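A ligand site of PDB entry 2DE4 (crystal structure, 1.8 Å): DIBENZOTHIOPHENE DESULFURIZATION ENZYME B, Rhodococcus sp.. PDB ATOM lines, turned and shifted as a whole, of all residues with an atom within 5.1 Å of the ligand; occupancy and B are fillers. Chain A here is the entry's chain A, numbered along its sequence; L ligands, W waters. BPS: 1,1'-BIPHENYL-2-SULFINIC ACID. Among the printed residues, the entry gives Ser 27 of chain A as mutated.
An oxygen (OX1) of the ligand lies within hydrogen-bond range of a ring nitrogen (NE2) of His 60, at 2.6 Å. An oxygen (OX1) of the ligand lies within salt-bridge range of the guanidinium group (NH2) of Arg 70. OX1 of the ligand sits at hydrogen-bond distance from OG of Ser 27. The backbone NH (N) of Gly 73 sits close to an oxygen (OX2) of the ligand, at 3.3 Å.
Water W1 lies within hydrogen-bond range of OX2 of the ligand (2.9 Å), N of Ile 75 (3.0 Å) and N of Glu 74 (3.4 Å).
Pro 28 touches the ligand. CZ of Phe 61 touches CX9 of the ligand, 3.5 Å away. CD of Pro 76 touches OX2 of the ligand (3.5 Å). CH2 of Trp 145 touches CXA of the ligand (3.98 Å). CD1 of Leu 152 touches CX8 of the ligand (3.7 Å). Trp 155 touches the ligand (CZ2 to CX4, 3.5 Å). Gly 183 touches the ligand. Leu 202 touches the ligand. Phe 203 touches the ligand (CZ to CXC, 3.7 Å). Trp 225 touches the ligand. Leu 226 touches the ligand (CD1 to CX6, 3.7 Å). CH2 of Trp 228 touches CX6 of the ligand, 3.9 Å away. Hydrophobic or aromatic side chains within 4 Å of the ligand: Pro 28, His 60, Phe 61, Pro 76, Trp 145, Leu 152, Trp 155, Leu 202, Phe 203, Trp 225, Leu 226 and Trp 228. Within 4 Å of the ligand: Ser 27, Pro 28, His 60, Phe 61, Arg 70, Gly 73, Pro 76, Trp 145, Leu 152, Trp 155, Gly 183, Leu 202, Phe 203, Trp 225, Leu 226 and Trp 228. The nearest printed residue that does not touch the ligand is Val 186 (4.3 Å).
NE1 of Trp 145 sits at hydrogen-bond distance from O of Val 186. O of His 60 is in hydrogen-bond range of NE of Arg 70 (3.1 Å). NH1 of Arg 70 lies within hydrogen-bond range of O of Gly 73, 2.9 Å away. N of Gly 73 is in hydrogen-bond range of OG of Ser 27, 3.0 Å away. OG of Ser 27 is in hydrogen-bond range of NH2 of Arg 70 (3.3 Å).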
ATOM      1  N   SER A  27      20.989  -4.893  20.443  1.00  0.00           N
ATOM      2  CA  SER A  27      20.416  -3.603  20.085  1.00  0.00           C
ATOM      3  C   SER A  27      21.433  -2.538  20.487  1.00  0.00           C
ATOM      4  O   SER A  27      22.446  -2.854  21.115  1.00  0.00           O
ATOM      5  CB  SER A  27      19.103  -3.374  20.839  1.00  0.00           C
ATOM      6  OG  SER A  27      18.195  -4.429  20.579  1.00  0.00           O
ATOM      7  N   PRO A  28      21.184  -1.270  20.125  1.00  0.00           N
ATOM      8  CA  PRO A  28      22.093  -0.179  20.475  1.00  0.00           C
ATOM      9  C   PRO A  28      21.943   0.150  21.959  1.00  0.00           C
ATOM     10  O   PRO A  28      21.570   1.268  22.323  1.00  0.00           O
ATOM     11  CB  PRO A  28      21.608   0.978  19.592  1.00  0.00           C
ATOM     12  CG  PRO A  28      20.937   0.299  18.441  1.00  0.00           C
ATOM     13  CD  PRO A  28      20.202  -0.838  19.119  1.00  0.00           C
ATOM     14  N   VAL A  29      22.223  -0.828  22.811  1.00  0.00           N
ATOM     15  CA  VAL A  29      22.093  -0.656  24.252  1.00  0.00           C
ATOM     16  C   VAL A  29      23.282  -1.268  24.988  1.00  0.00           C
ATOM     17  O   VAL A  29      23.962  -2.149  24.448  1.00  0.00           O
ATOM     18  CB  VAL A  29      20.790  -1.327  24.774  1.00  0.00           C
ATOM     19  CG1 VAL A  29      19.587  -0.811  24.001  1.00  0.00           C
ATOM     20  CG2 VAL A  29      20.893  -2.840  24.629  1.00  0.00           C
ATOM     21  N   HIS A  60      16.366 -10.943  14.462  1.00  0.00           N
ATOM     22  CA  HIS A  60      16.507 -10.012  15.579  1.00  0.00           C
ATOM     23  C   HIS A  60      15.130  -9.771  16.190  1.00  0.00           C
ATOM     24  O   HIS A  60      15.024  -9.404  17.357  1.00  0.00           O
ATOM     25  CB  HIS A  60      17.100  -8.695  15.057  1.00  0.00           C
ATOM     26  CG  HIS A  60      17.431  -7.693  16.135  1.00  0.00           C
ATOM     27  ND1 HIS A  60      18.524  -7.819  16.955  1.00  0.00           N
ATOM     28  CD2 HIS A  60      16.824  -6.543  16.491  1.00  0.00           C
ATOM     29  CE1 HIS A  60      18.587  -6.784  17.773  1.00  0.00           C
ATOM     30  NE2 HIS A  60      17.564  -5.993  17.511  1.00  0.00           N
ATOM     31  N   PHE A  61      14.086  -9.982  15.388  1.00  0.00           N
ATOM     32  CA  PHE A  61      12.696  -9.807  15.824  1.00  0.00           C
ATOM     33  C   PHE A  61      11.928 -11.127  15.927  1.00  0.00           C
ATOM     34  O   PHE A  61      10.932 -11.197  16.661  1.00  0.00           O
ATOM     35  CB  PHE A  61      11.903  -8.936  14.835  1.00  0.00           C
ATOM     36  CG  PHE A  61      12.187  -7.458  14.929  1.00  0.00           C
ATOM     37  CD1 PHE A  61      13.202  -6.950  15.740  1.00  0.00           C
ATOM     38  CD2 PHE A  61      11.440  -6.573  14.153  1.00  0.00           C
ATOM     39  CE1 PHE A  61      13.465  -5.586  15.772  1.00  0.00           C
ATOM     40  CE2 PHE A  61      11.697  -5.200  14.177  1.00  0.00           C
ATOM     41  CZ  PHE A  61      12.710  -4.707  14.986  1.00  0.00           C
ATOM     42  N   ARG A  70      20.392 -13.045  21.757  1.00  0.00           N
ATOM     43  CA  ARG A  70      20.262 -11.611  21.546  1.00  0.00           C
ATOM     44  C   ARG A  70      20.177 -10.879  22.870  1.00  0.00           C
ATOM     45  O   ARG A  70      19.623 -11.389  23.842  1.00  0.00           O
ATOM     46  CB  ARG A  70      18.989 -11.327  20.745  1.00  0.00           C
ATOM     47  CG  ARG A  70      18.552  -9.854  20.674  1.00  0.00           C
ATOM     48  CD  ARG A  70      17.215  -9.767  19.952  1.00  0.00           C
ATOM     49  NE  ARG A  70      16.701  -8.412  19.759  1.00  0.00           N
ATOM     50  CZ  ARG A  70      16.125  -7.673  20.707  1.00  0.00           C
ATOM     51  NH1 ARG A  70      15.987  -8.136  21.941  1.00  0.00           N
ATOM     52  NH2 ARG A  70      15.640  -6.471  20.400  1.00  0.00           N
ATOM     53  N   GLY A  72      19.035  -7.113  23.753  1.00  0.00           N
ATOM     54  CA  GLY A  72      18.576  -5.829  23.250  1.00  0.00           C
ATOM     55  C   GLY A  72      17.242  -5.398  23.814  1.00  0.00           C
ATOM     56  O   GLY A  72      16.809  -5.879  24.859  1.00  0.00           O
ATOM     57  N   GLY A  73      16.586  -4.473  23.110  1.00  0.00           N
ATOM     58  CA  GLY A  73      15.290  -3.960  23.548  1.00  0.00           C
ATOM     59  C   GLY A  73      14.294  -5.088  23.782  1.00  0.00           C
ATOM     60  O   GLY A  73      14.303  -6.075  23.068  1.00  0.00           O
ATOM     61  N   GLU A  74      13.431  -4.900  24.776  1.00  0.00           N
ATOM     62  CA  GLU A  74      12.455  -5.919  25.146  1.00  0.00           C
ATOM     63  C   GLU A  74      11.186  -6.019  24.304  1.00  0.00           C
ATOM     64  O   GLU A  74      10.462  -7.008  24.394  1.00  0.00           O
ATOM     65  CB  GLU A  74      12.036  -5.738  26.606  1.00  0.00           C
ATOM     66  CG  GLU A  74      11.256  -4.445  26.872  1.00  0.00           C
ATOM     67  CD  GLU A  74      12.130  -3.293  27.340  1.00  0.00           C
ATOM     68  OE1 GLU A  74      13.107  -2.952  26.639  1.00  0.00           O
ATOM     69  OE2 GLU A  74      11.829  -2.721  28.413  1.00  0.00           O
ATOM     70  N   ILE A  75      10.888  -5.013  23.493  1.00  0.00           N
ATOM     71  CA  ILE A  75       9.659  -5.065  22.723  1.00  0.00           C
ATOM     72  C   ILE A  75       9.601  -6.199  21.683  1.00  0.00           C
ATOM     73  O   ILE A  75       8.617  -6.937  21.639  1.00  0.00           O
ATOM     74  CB  ILE A  75       9.358  -3.706  22.077  1.00  0.00           C
ATOM     75  CG1 ILE A  75       9.146  -2.671  23.198  1.00  0.00           C
ATOM     76  CG2 ILE A  75       8.112  -3.792  21.199  1.00  0.00           C
ATOM     77  CD1 ILE A  75       8.897  -1.243  22.702  1.00  0.00           C
ATOM     78  N   PRO A  76      10.653  -6.359  20.855  1.00  0.00           N
ATOM     79  CA  PRO A  76      10.565  -7.443  19.873  1.00  0.00           C
ATOM     80  C   PRO A  76      10.414  -8.827  20.506  1.00  0.00           C
ATOM     81  O   PRO A  76       9.553  -9.618  20.077  1.00  0.00           O
ATOM     82  CB  PRO A  76      11.873  -7.297  19.085  1.00  0.00           C
ATOM     83  CG  PRO A  76      12.128  -5.791  19.149  1.00  0.00           C
ATOM     84  CD  PRO A  76      11.821  -5.504  20.609  1.00  0.00           C
ATOM     85  N   TRP A 145       8.134  -8.444  10.979  1.00  0.00           N
ATOM     86  CA  TRP A 145       9.019  -7.286  10.934  1.00  0.00           C
ATOM     87  C   TRP A 145       8.263  -5.968  11.016  1.00  0.00           C
ATOM     88  O   TRP A 145       8.551  -5.139  11.892  1.00  0.00           O
ATOM     89  CB  TRP A 145       9.888  -7.305   9.675  1.00  0.00           C
ATOM     90  CG  TRP A 145      10.937  -6.229   9.674  1.00  0.00           C
ATOM     91  CD1 TRP A 145      10.901  -5.046   8.996  1.00  0.00           C
ATOM     92  CD2 TRP A 145      12.152  -6.224  10.430  1.00  0.00           C
ATOM     93  NE1 TRP A 145      12.017  -4.301   9.283  1.00  0.00           N
ATOM     94  CE2 TRP A 145      12.806  -5.005  10.158  1.00  0.00           C
ATOM     95  CE3 TRP A 145      12.762  -7.133  11.306  1.00  0.00           C
ATOM     96  CZ2 TRP A 145      14.029  -4.659  10.737  1.00  0.00           C
ATOM     97  CZ3 TRP A 145      13.985  -6.787  11.884  1.00  0.00           C
ATOM     98  CH2 TRP A 145      14.601  -5.562  11.602  1.00  0.00           C
ATOM     99  N   LEU A 149       7.788  -3.185  14.195  1.00  0.00           N
ATOM    100  CA  LEU A 149       8.135  -1.779  13.995  1.00  0.00           C
ATOM    101  C   LEU A 149       7.013  -0.847  14.453  1.00  0.00           C
ATOM    102  O   LEU A 149       7.276   0.275  14.875  1.00  0.00           O
ATOM    103  CB  LEU A 149       8.479  -1.513  12.520  1.00  0.00           C
ATOM    104  CG  LEU A 149       9.763  -2.170  12.008  1.00  0.00           C
ATOM    105  CD1 LEU A 149      10.010  -1.721  10.570  1.00  0.00           C
ATOM    106  CD2 LEU A 149      10.953  -1.776  12.880  1.00  0.00           C
ATOM    107  N   LEU A 152       7.406  -0.532  18.126  1.00  0.00           N
ATOM    108  CA  LEU A 152       8.565   0.249  18.538  1.00  0.00           C
ATOM    109  C   LEU A 152       8.221   1.736  18.591  1.00  0.00           C
ATOM    110  O   LEU A 152       9.015   2.555  19.053  1.00  0.00           O
ATOM    111  CB  LEU A 152       9.752   0.001  17.592  1.00  0.00           C
ATOM    112  CG  LEU A 152      10.281  -1.444  17.609  1.00  0.00           C
ATOM    113  CD1 LEU A 152      11.603  -1.525  16.869  1.00  0.00           C
ATOM    114  CD2 LEU A 152      10.470  -1.902  19.063  1.00  0.00           C
ATOM    115  N   TRP A 155       8.328   3.924  22.213  1.00  0.00           N
ATOM    116  CA  TRP A 155       9.309   4.798  22.857  1.00  0.00           C
ATOM    117  C   TRP A 155       8.883   6.258  22.744  1.00  0.00           C
ATOM    118  O   TRP A 155       8.874   6.997  23.730  1.00  0.00           O
ATOM    119  CB  TRP A 155      10.687   4.639  22.211  1.00  0.00           C
ATOM    120  CG  TRP A 155      11.187   3.217  22.162  1.00  0.00           C
ATOM    121  CD1 TRP A 155      11.139   2.287  23.156  1.00  0.00           C
ATOM    122  CD2 TRP A 155      11.895   2.613  21.080  1.00  0.00           C
ATOM    123  NE1 TRP A 155      11.778   1.128  22.758  1.00  0.00           N
ATOM    124  CE2 TRP A 155      12.249   1.306  21.493  1.00  0.00           C
ATOM    125  CE3 TRP A 155      12.272   3.054  19.804  1.00  0.00           C
ATOM    126  CZ2 TRP A 155      12.970   0.432  20.664  1.00  0.00           C
ATOM    127  CZ3 TRP A 155      12.980   2.181  18.986  1.00  0.00           C
ATOM    128  CH2 TRP A 155      13.320   0.882  19.417  1.00  0.00           C
ATOM    129  N   GLY A 183      15.292   3.228  14.114  1.00  0.00           N
ATOM    130  CA  GLY A 183      14.890   1.985  14.745  1.00  0.00           C
ATOM    131  C   GLY A 183      13.416   1.678  14.589  1.00  0.00           C
ATOM    132  O   GLY A 183      12.978   0.550  14.779  1.00  0.00           O
ATOM    133  N   VAL A 186      12.473   1.272   9.509  1.00  0.00           N
ATOM    134  CA  VAL A 186      13.533   0.448   8.956  1.00  0.00           C
ATOM    135  C   VAL A 186      12.950  -0.434   7.868  1.00  0.00           C
ATOM    136  O   VAL A 186      12.515  -1.560   8.125  1.00  0.00           O
ATOM    137  CB  VAL A 186      14.159  -0.450  10.043  1.00  0.00           C
ATOM    138  CG1 VAL A 186      15.382  -1.174   9.489  1.00  0.00           C
ATOM    139  CG2 VAL A 186      14.538   0.385  11.270  1.00  0.00           C
ATOM    140  N   LEU A 202      23.378  -0.665  10.432  1.00  0.00           N
ATOM    141  CA  LEU A 202      21.953  -0.428  10.286  1.00  0.00           C
ATOM    142  C   LEU A 202      21.468   0.979  10.612  1.00  0.00           C
ATOM    143  O   LEU A 202      20.501   1.465  10.024  1.00  0.00           O
ATOM    144  CB  LEU A 202      21.185  -1.452  11.143  1.00  0.00           C
ATOM    145  CG  LEU A 202      19.689  -1.643  10.903  1.00  0.00           C
ATOM    146  CD1 LEU A 202      19.448  -2.102   9.470  1.00  0.00           C
ATOM    147  CD2 LEU A 202      19.166  -2.680  11.889  1.00  0.00           C
ATOM    148  N   PHE A 203      22.143   1.638  11.550  1.00  0.00           N
ATOM    149  CA  PHE A 203      21.750   2.991  11.967  1.00  0.00           C
ATOM    150  C   PHE A 203      22.895   3.991  11.844  1.00  0.00           C
ATOM    151  O   PHE A 203      23.338   4.568  12.853  1.00  0.00           O
ATOM    152  CB  PHE A 203      21.250   2.954  13.411  1.00  0.00           C
ATOM    153  CG  PHE A 203      20.158   1.961  13.645  1.00  0.00           C
ATOM    154  CD1 PHE A 203      18.947   2.070  12.975  1.00  0.00           C
ATOM    155  CD2 PHE A 203      20.343   0.893  14.525  1.00  0.00           C
ATOM    156  CE1 PHE A 203      17.926   1.127  13.172  1.00  0.00           C
ATOM    157  CE2 PHE A 203      19.341  -0.046  14.735  1.00  0.00           C
ATOM    158  CZ  PHE A 203      18.133   0.064  14.051  1.00  0.00           C
ATOM    159  N   TRP A 225      17.097   9.467  21.828  1.00  0.00           N
ATOM    160  CA  TRP A 225      17.603   8.807  23.021  1.00  0.00           C
ATOM    161  C   TRP A 225      18.812   7.974  22.606  1.00  0.00           C
ATOM    162  O   TRP A 225      19.255   8.061  21.463  1.00  0.00           O
ATOM    163  CB  TRP A 225      16.497   7.917  23.622  1.00  0.00           C
ATOM    164  CG  TRP A 225      16.072   6.763  22.754  1.00  0.00           C
ATOM    165  CD1 TRP A 225      15.984   6.743  21.388  1.00  0.00           C
ATOM    166  CD2 TRP A 225      15.651   5.464  23.201  1.00  0.00           C
ATOM    167  NE1 TRP A 225      15.550   5.516  20.957  1.00  0.00           N
ATOM    168  CE2 TRP A 225      15.346   4.707  22.050  1.00  0.00           C
ATOM    169  CE3 TRP A 225      15.527   4.862  24.457  1.00  0.00           C
ATOM    170  CZ2 TRP A 225      14.902   3.375  22.114  1.00  0.00           C
ATOM    171  CZ3 TRP A 225      15.085   3.543  24.522  1.00  0.00           C
ATOM    172  CH2 TRP A 225      14.787   2.822  23.366  1.00  0.00           C
ATOM    173  N   LEU A 226      19.348   7.171  23.538  1.00  0.00           N
ATOM    174  CA  LEU A 226      20.522   6.355  23.254  1.00  0.00           C
ATOM    175  C   LEU A 226      21.683   7.298  22.898  1.00  0.00           C
ATOM    176  O   LEU A 226      21.567   8.509  23.074  1.00  0.00           O
ATOM    177  CB  LEU A 226      20.231   5.389  22.092  1.00  0.00           C
ATOM    178  CG  LEU A 226      18.938   4.588  22.215  1.00  0.00           C
ATOM    179  CD1 LEU A 226      18.857   3.556  21.090  1.00  0.00           C
ATOM    180  CD2 LEU A 226      18.897   3.889  23.572  1.00  0.00           C
ATOM    181  N   TRP A 228      22.518   8.329  20.220  1.00  0.00           N
ATOM    182  CA  TRP A 228      22.069   9.214  19.170  1.00  0.00           C
ATOM    183  C   TRP A 228      21.703  10.580  19.757  1.00  0.00           C
ATOM    184  O   TRP A 228      22.024  11.622  19.191  1.00  0.00           O
ATOM    185  CB  TRP A 228      20.845   8.613  18.458  1.00  0.00           C
ATOM    186  CG  TRP A 228      21.077   7.219  17.920  1.00  0.00           C
ATOM    187  CD1 TRP A 228      22.236   6.714  17.413  1.00  0.00           C
ATOM    188  CD2 TRP A 228      20.087   6.188  17.776  1.00  0.00           C
ATOM    189  NE1 TRP A 228      22.047   5.419  16.970  1.00  0.00           N
ATOM    190  CE2 TRP A 228      20.737   5.072  17.177  1.00  0.00           C
ATOM    191  CE3 TRP A 228      18.730   6.082  18.095  1.00  0.00           C
ATOM    192  CZ2 TRP A 228      20.060   3.881  16.883  1.00  0.00           C
ATOM    193  CZ3 TRP A 228      18.055   4.899  17.795  1.00  0.00           C
ATOM    194  CH2 TRP A 228      18.727   3.814  17.210  1.00  0.00           C
HETATM  195  CX1 BPS L   1      16.965   0.204  17.982  1.00  0.00           C
HETATM  196  CX2 BPS L   1      16.393  -1.070  17.974  1.00  0.00           C
HETATM  197  CX3 BPS L   1      15.972  -1.658  19.173  1.00  0.00           C
HETATM  198  CX4 BPS L   1      16.139  -0.957  20.371  1.00  0.00           C
HETATM  199  CX5 BPS L   1      16.712   0.311  20.372  1.00  0.00           C
HETATM  200  CX6 BPS L   1      17.130   0.891  19.179  1.00  0.00           C
HETATM  201  CX7 BPS L   1      16.307  -1.745  16.763  1.00  0.00           C
HETATM  202  CX8 BPS L   1      15.214  -1.532  15.917  1.00  0.00           C
HETATM  203  CX9 BPS L   1      15.118  -2.198  14.711  1.00  0.00           C
HETATM  204  CXA BPS L   1      16.120  -3.091  14.324  1.00  0.00           C
HETATM  205  CXB BPS L   1      17.214  -3.311  15.163  1.00  0.00           C
HETATM  206  CXC BPS L   1      17.310  -2.638  16.376  1.00  0.00           C
HETATM  207  SX1 BPS L   1      15.224  -3.234  19.215  1.00  0.00           S
HETATM  208  OX1 BPS L   1      16.188  -4.242  18.901  1.00  0.00           O
HETATM  209  OX2 BPS L   1      14.676  -3.530  20.578  1.00  0.00           O
HETATM  210  O   HOH W   1      12.463  -2.799  22.290  1.00  0.00           O
